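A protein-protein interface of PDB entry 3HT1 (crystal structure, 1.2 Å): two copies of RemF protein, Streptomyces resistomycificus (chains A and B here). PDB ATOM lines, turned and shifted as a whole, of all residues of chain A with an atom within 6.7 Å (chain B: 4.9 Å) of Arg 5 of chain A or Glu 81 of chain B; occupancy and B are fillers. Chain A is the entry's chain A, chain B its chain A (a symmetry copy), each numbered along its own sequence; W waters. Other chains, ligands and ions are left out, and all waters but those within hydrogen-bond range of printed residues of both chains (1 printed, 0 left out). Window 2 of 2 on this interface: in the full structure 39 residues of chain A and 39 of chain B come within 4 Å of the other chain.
O of Glu 82 of chain B lies within hydrogen-bond range of NH1 of Arg 5 of chain A, 3.3 Å away.
The side-chain carboxylate (OE1) of Glu 87 of chain B is in salt-bridge range of the guanidinium group (NH1) of Arg 5 of chain A, at 3.0 Å.
NH2 of Arg 5 of chain A is in salt-bridge range of OE2 of Glu 81 of chain B, at 3.5 Å.
The backbone NH (N) of Ala 88 of chain B sits at hydrogen-bond distance from the backbone carbonyl oxygen (O) of Val 6 of chain A.
N of Leu 74 of chain B lies within hydrogen-bond range of O of Arg 79 of chain B (2.8 Å).
The backbone NH of Leu 72 of chain B lies within hydrogen-bond range of the backbone carbonyl oxygen of Glu 81 of chain B, 2.8 Å away.
NH2 of Arg 79 of chain B lies within salt-bridge range of OE1 of Glu 81 of chain B (2.7 Å).
Leu 72 of chain B touches Met 3 of chain A.
Met 3 of chain A touches Leu 74 of chain B (SD to CD2, 3.9 Å).
Ile 89 of chain B touches Met 3 of chain A (CG2 to SD, 3.96 Å).
Lys 4 of chain A touches Ala 88 of chain B (O to O, 3.8 Å).
CA of Ile 89 of chain B touches O of Lys 4 of chain A, at 3.2 Å.
Ala 88 of chain B touches Arg 5 of chain A.
Glu 87 of chain B touches Val 6 of chain A (CA to O, 3.4 Å).
His 7 of chain A touches Glu 87 of chain B.
Of the printed residues of chain B, Arg 5 of chain A touches Glu 81 (3.3 Å), Glu 82 (3.3 Å), Glu 87 (3.0 Å) and Ala 88 (3.4 Å).
Printed residues of chain A within 4 Å of Glu 81 of chain B: Arg 5.
Of the printed residues of chain B, Met 3 of chain A touches Leu 72, Leu 74 and Ile 89.
Of the printed residues of chain B, His 7 of chain A touches Glu 87.
Of the printed residues of chain A, Ala 88 of chain B touches Lys 4, Arg 5 and Val 6.
The nearest printed residue of chain B that does not touch Met 3 of chain A is Arg 79 of chain B (6.3 Å).
Of the 5 printed residues of chain A, 5 touch a printed residue of chain B.
Printed residues of chain A that touch a printed residue of chain B: Met 3, Lys 4, Arg 5, Val 6 and His 7.
Along chain A the printed residues that touch a printed residue of chain B span positions 3 to 7.
Hydrophobic or aromatic side chains of chain B within 4 Å of the printed part of chain A: Leu 72, Leu 74, Ala 88 and Ile 89.
Among the printed residues, 12 pairs touch across the chains.
No position is printed for both chains.
Water W1 lies within hydrogen-bond range of the side-chain carboxylate of Glu 87 of chain B, the backbone carbonyl oxygen of Glu 82 of chain B and the guanidinium group of Arg 5 of chain A.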
ATOM      1  N   MET A   3      -3.210 -31.083  10.617  1.00  0.00           N
ATOM      2  CA  MET A   3      -4.593 -30.737  11.064  1.00  0.00           C
ATOM      3  C   MET A   3      -5.326 -30.290   9.794  1.00  0.00           C
ATOM      4  O   MET A   3      -4.753 -29.446   9.073  1.00  0.00           O
ATOM      5  CB  MET A   3      -4.569 -29.687  12.165  1.00  0.00           C
ATOM      6  CG  MET A   3      -5.248 -29.499  13.485  1.00  0.00           C
ATOM      7  SD  MET A   3      -6.835 -28.747  13.334  1.00  0.00           S
ATOM      8  CE  MET A   3      -7.112 -28.157  11.703  1.00  0.00           C
ATOM      9  N   LYS A   4      -6.512 -30.808   9.482  1.00  0.00           N
ATOM     10  CA  LYS A   4      -7.376 -30.512   8.333  1.00  0.00           C
ATOM     11  C   LYS A   4      -8.691 -29.951   8.862  1.00  0.00           C
ATOM     12  O   LYS A   4      -9.286 -30.578   9.735  1.00  0.00           O
ATOM     13  CB  LYS A   4      -7.696 -31.724   7.414  1.00  0.00           C
ATOM     14  CG  LYS A   4      -8.750 -31.511   6.324  1.00  0.00           C
ATOM     15  CD  LYS A   4      -9.424 -32.725   5.689  1.00  0.00           C
ATOM     16  CE  LYS A   4      -9.916 -32.622   4.268  1.00  0.00           C
ATOM     17  NZ  LYS A   4     -10.427 -33.868   3.622  1.00  0.00           N
ATOM     18  N   ARG A   5      -9.168 -28.848   8.349  1.00  0.00           N
ATOM     19  CA  ARG A   5     -10.477 -28.287   8.583  1.00  0.00           C
ATOM     20  C   ARG A   5     -11.111 -28.082   7.209  1.00  0.00           C
ATOM     21  O   ARG A   5     -10.530 -27.351   6.403  1.00  0.00           O
ATOM     22  CB  ARG A   5     -10.569 -26.948   9.330  1.00  0.00           C
ATOM     23  CG  ARG A   5     -12.008 -26.507   9.596  1.00  0.00           C
ATOM     24  CD  ARG A   5     -12.773 -25.637   8.584  1.00  0.00           C
ATOM     25  NE  ARG A   5     -11.881 -24.458   8.407  1.00  0.00           N
ATOM     26  CZ  ARG A   5     -11.999 -23.323   9.071  1.00  0.00           C
ATOM     27  NH1 ARG A   5     -12.949 -23.104   9.987  1.00  0.00           N
ATOM     28  NH2 ARG A   5     -11.081 -22.387   8.770  1.00  0.00           N
ATOM     29  N   VAL A   6     -12.287 -28.664   6.993  1.00  0.00           N
ATOM     30  CA  VAL A   6     -12.954 -28.432   5.688  1.00  0.00           C
ATOM     31  C   VAL A   6     -14.454 -28.331   5.930  1.00  0.00           C
ATOM     32  O   VAL A   6     -15.030 -29.059   6.739  1.00  0.00           O
ATOM     33  CB  VAL A   6     -12.586 -29.526   4.680  1.00  0.00           C
ATOM     34  CG1 VAL A   6     -13.114 -30.870   5.104  1.00  0.00           C
ATOM     35  CG2 VAL A   6     -13.073 -29.147   3.286  1.00  0.00           C
ATOM     36  N   HIS A   7     -15.114 -27.428   5.217  1.00  0.00           N
ATOM     37  CA  HIS A   7     -16.553 -27.359   5.266  1.00  0.00           C
ATOM     38  C   HIS A   7     -17.109 -28.404   4.327  1.00  0.00           C
ATOM     39  O   HIS A   7     -16.569 -28.629   3.242  1.00  0.00           O
ATOM     40  CB  HIS A   7     -17.071 -25.936   4.857  1.00  0.00           C
ATOM     41  CG  HIS A   7     -18.517 -25.813   5.182  1.00  0.00           C
ATOM     42  ND1 HIS A   7     -19.109 -25.639   6.398  1.00  0.00           N
ATOM     43  CD2 HIS A   7     -19.532 -25.870   4.258  1.00  0.00           C
ATOM     44  CE1 HIS A   7     -20.436 -25.615   6.163  1.00  0.00           C
ATOM     45  NE2 HIS A   7     -20.715 -25.771   4.873  1.00  0.00           N
ATOM     46  N   MET B  70     -17.557 -22.253  17.886  1.00  0.00           N
ATOM     47  CA  MET B  70     -16.611 -22.234  18.986  1.00  0.00           C
ATOM     48  C   MET B  70     -15.236 -21.965  18.391  1.00  0.00           C
ATOM     49  O   MET B  70     -15.064 -22.007  17.173  1.00  0.00           O
ATOM     50  CB  MET B  70     -16.593 -23.568  19.727  1.00  0.00           C
ATOM     51  CG  MET B  70     -16.164 -24.736  18.871  1.00  0.00           C
ATOM     52  SD  MET B  70     -16.217 -26.287  19.813  1.00  0.00           S
ATOM     53  CE  MET B  70     -15.780 -27.405  18.459  1.00  0.00           C
ATOM     54  N   GLY B  71     -14.285 -21.758  19.279  1.00  0.00           N
ATOM     55  CA  GLY B  71     -12.894 -21.661  18.875  1.00  0.00           C
ATOM     56  C   GLY B  71     -12.177 -22.985  19.076  1.00  0.00           C
ATOM     57  O   GLY B  71     -12.299 -23.599  20.127  1.00  0.00           O
ATOM     58  N   LEU B  72     -11.431 -23.395  18.088  1.00  0.00           N
ATOM     59  CA  LEU B  72     -10.487 -24.488  18.144  1.00  0.00           C
ATOM     60  C   LEU B  72      -9.118 -23.852  18.436  1.00  0.00           C
ATOM     61  O   LEU B  72      -8.548 -23.196  17.532  1.00  0.00           O
ATOM     62  CB  LEU B  72     -10.496 -25.259  16.838  1.00  0.00           C
ATOM     63  CG  LEU B  72      -9.431 -26.317  16.649  1.00  0.00           C
ATOM     64  CD1 LEU B  72      -9.429 -27.395  17.729  1.00  0.00           C
ATOM     65  CD2 LEU B  72      -9.565 -26.934  15.253  1.00  0.00           C
ATOM     66  N   LEU B  74      -5.275 -23.720  18.924  1.00  0.00           N
ATOM     67  CA  LEU B  74      -4.208 -24.442  18.251  1.00  0.00           C
ATOM     68  C   LEU B  74      -2.881 -23.916  18.730  1.00  0.00           C
ATOM     69  O   LEU B  74      -2.265 -23.017  18.110  1.00  0.00           O
ATOM     70  CB  LEU B  74      -4.363 -24.293  16.724  1.00  0.00           C
ATOM     71  CG  LEU B  74      -5.632 -24.993  16.170  1.00  0.00           C
ATOM     72  CD1 LEU B  74      -5.860 -24.482  14.743  1.00  0.00           C
ATOM     73  CD2 LEU B  74      -5.532 -26.490  16.250  1.00  0.00           C
ATOM     74  N   ARG B  79      -2.739 -19.608  17.609  1.00  0.00           N
ATOM     75  CA  ARG B  79      -4.034 -18.954  17.369  1.00  0.00           C
ATOM     76  C   ARG B  79      -5.191 -19.908  17.654  1.00  0.00           C
ATOM     77  O   ARG B  79      -5.001 -21.033  18.100  1.00  0.00           O
ATOM     78  CB  ARG B  79      -4.186 -18.425  15.927  1.00  0.00           C
ATOM     79  CG  ARG B  79      -4.465 -19.625  15.024  1.00  0.00           C
ATOM     80  CD  ARG B  79      -4.140 -19.419  13.549  1.00  0.00           C
ATOM     81  NE  ARG B  79      -4.515 -20.619  12.819  1.00  0.00           N
ATOM     82  CZ  ARG B  79      -5.669 -20.847  12.219  1.00  0.00           C
ATOM     83  NH1 ARG B  79      -6.656 -19.961  12.200  1.00  0.00           N
ATOM     84  NH2 ARG B  79      -5.888 -21.998  11.598  1.00  0.00           N
ATOM     85  N   THR B  80      -6.389 -19.392  17.422  1.00  0.00           N
ATOM     86  CA  THR B  80      -7.659 -20.048  17.640  1.00  0.00           C
ATOM     87  C   THR B  80      -8.466 -19.838  16.367  1.00  0.00           C
ATOM     88  O   THR B  80      -8.586 -18.739  15.867  1.00  0.00           O
ATOM     89  CB  THR B  80      -8.411 -19.444  18.817  1.00  0.00           C
ATOM     90  OG1 THR B  80      -7.670 -19.640  20.012  1.00  0.00           O
ATOM     91  CG2 THR B  80      -9.774 -20.071  19.050  1.00  0.00           C
ATOM     92  N   GLU B  81      -8.954 -20.914  15.810  1.00  0.00           N
ATOM     93  CA  GLU B  81      -9.757 -20.978  14.615  1.00  0.00           C
ATOM     94  C   GLU B  81     -11.240 -21.035  14.956  1.00  0.00           C
ATOM     95  O   GLU B  81     -11.620 -21.983  15.627  1.00  0.00           O
ATOM     96  CB  GLU B  81      -9.360 -22.224  13.820  1.00  0.00           C
ATOM     97  CG  GLU B  81     -10.050 -22.336  12.455  1.00  0.00           C
ATOM     98  CD  GLU B  81      -9.566 -21.266  11.496  1.00  0.00           C
ATOM     99  OE1 GLU B  81      -8.506 -21.668  10.979  1.00  0.00           O
ATOM    100  OE2 GLU B  81     -10.201 -20.214  11.303  1.00  0.00           O
ATOM    101  N   GLU B  82     -12.069 -20.111  14.468  1.00  0.00           N
ATOM    102  CA  GLU B  82     -13.501 -20.234  14.718  1.00  0.00           C
ATOM    103  C   GLU B  82     -14.018 -21.281  13.770  1.00  0.00           C
ATOM    104  O   GLU B  82     -13.768 -21.259  12.554  1.00  0.00           O
ATOM    105  CB  GLU B  82     -14.226 -18.889  14.578  1.00  0.00           C
ATOM    106  CG  GLU B  82     -13.975 -17.928  15.755  1.00  0.00           C
ATOM    107  CD  GLU B  82     -14.479 -18.348  17.123  1.00  0.00           C
ATOM    108  OE1 GLU B  82     -15.688 -18.606  17.305  1.00  0.00           O
ATOM    109  OE2 GLU B  82     -13.710 -18.432  18.101  1.00  0.00           O
ATOM    110  N   VAL B  83     -14.754 -22.221  14.295  1.00  0.00           N
ATOM    111  CA  VAL B  83     -15.385 -23.285  13.545  1.00  0.00           C
ATOM    112  C   VAL B  83     -16.884 -23.162  13.762  1.00  0.00           C
ATOM    113  O   VAL B  83     -17.409 -22.674  14.735  1.00  0.00           O
ATOM    114  CB  VAL B  83     -14.824 -24.680  13.899  1.00  0.00           C
ATOM    115  CG1 VAL B  83     -13.333 -24.772  13.603  1.00  0.00           C
ATOM    116  CG2 VAL B  83     -15.141 -25.034  15.346  1.00  0.00           C
ATOM    117  N   GLU B  87     -18.581 -28.181   9.480  1.00  0.00           N
ATOM    118  CA  GLU B  87     -17.137 -28.339   9.353  1.00  0.00           C
ATOM    119  C   GLU B  87     -16.700 -29.685   9.915  1.00  0.00           C
ATOM    120  O   GLU B  87     -17.089 -30.101  10.982  1.00  0.00           O
ATOM    121  CB  GLU B  87     -16.443 -27.172  10.053  1.00  0.00           C
ATOM    122  CG  GLU B  87     -16.759 -25.899   9.180  1.00  0.00           C
ATOM    123  CD  GLU B  87     -16.146 -24.688   9.858  1.00  0.00           C
ATOM    124  OE1 GLU B  87     -15.213 -24.907  10.622  1.00  0.00           O
ATOM    125  OE2 GLU B  87     -16.678 -23.608   9.601  1.00  0.00           O
ATOM    126  N   ALA B  88     -15.812 -30.322   9.139  1.00  0.00           N
ATOM    127  CA  ALA B  88     -15.136 -31.545   9.508  1.00  0.00           C
ATOM    128  C   ALA B  88     -13.673 -31.228   9.828  1.00  0.00           C
ATOM    129  O   ALA B  88     -13.047 -30.502   9.108  1.00  0.00           O
ATOM    130  CB  ALA B  88     -15.213 -32.605   8.414  1.00  0.00           C
ATOM    131  N   ILE B  89     -13.199 -31.733  10.949  1.00  0.00           N
ATOM    132  CA  ILE B  89     -11.881 -31.442  11.444  1.00  0.00           C
ATOM    133  C   ILE B  89     -11.147 -32.734  11.781  1.00  0.00           C
ATOM    134  O   ILE B  89     -11.649 -33.560  12.528  1.00  0.00           O
ATOM    135  CB  ILE B  89     -11.935 -30.535  12.671  1.00  0.00           C
ATOM    136  CG1 ILE B  89     -12.755 -29.266  12.448  1.00  0.00           C
ATOM    137  CG2 ILE B  89     -10.513 -30.213  13.132  1.00  0.00           C
ATOM    138  CD1 ILE B  89     -13.231 -28.559  13.701  1.00  0.00           C
HETATM  139  O   HOH W   1     -15.827 -21.264  10.495  1.00  0.00           O
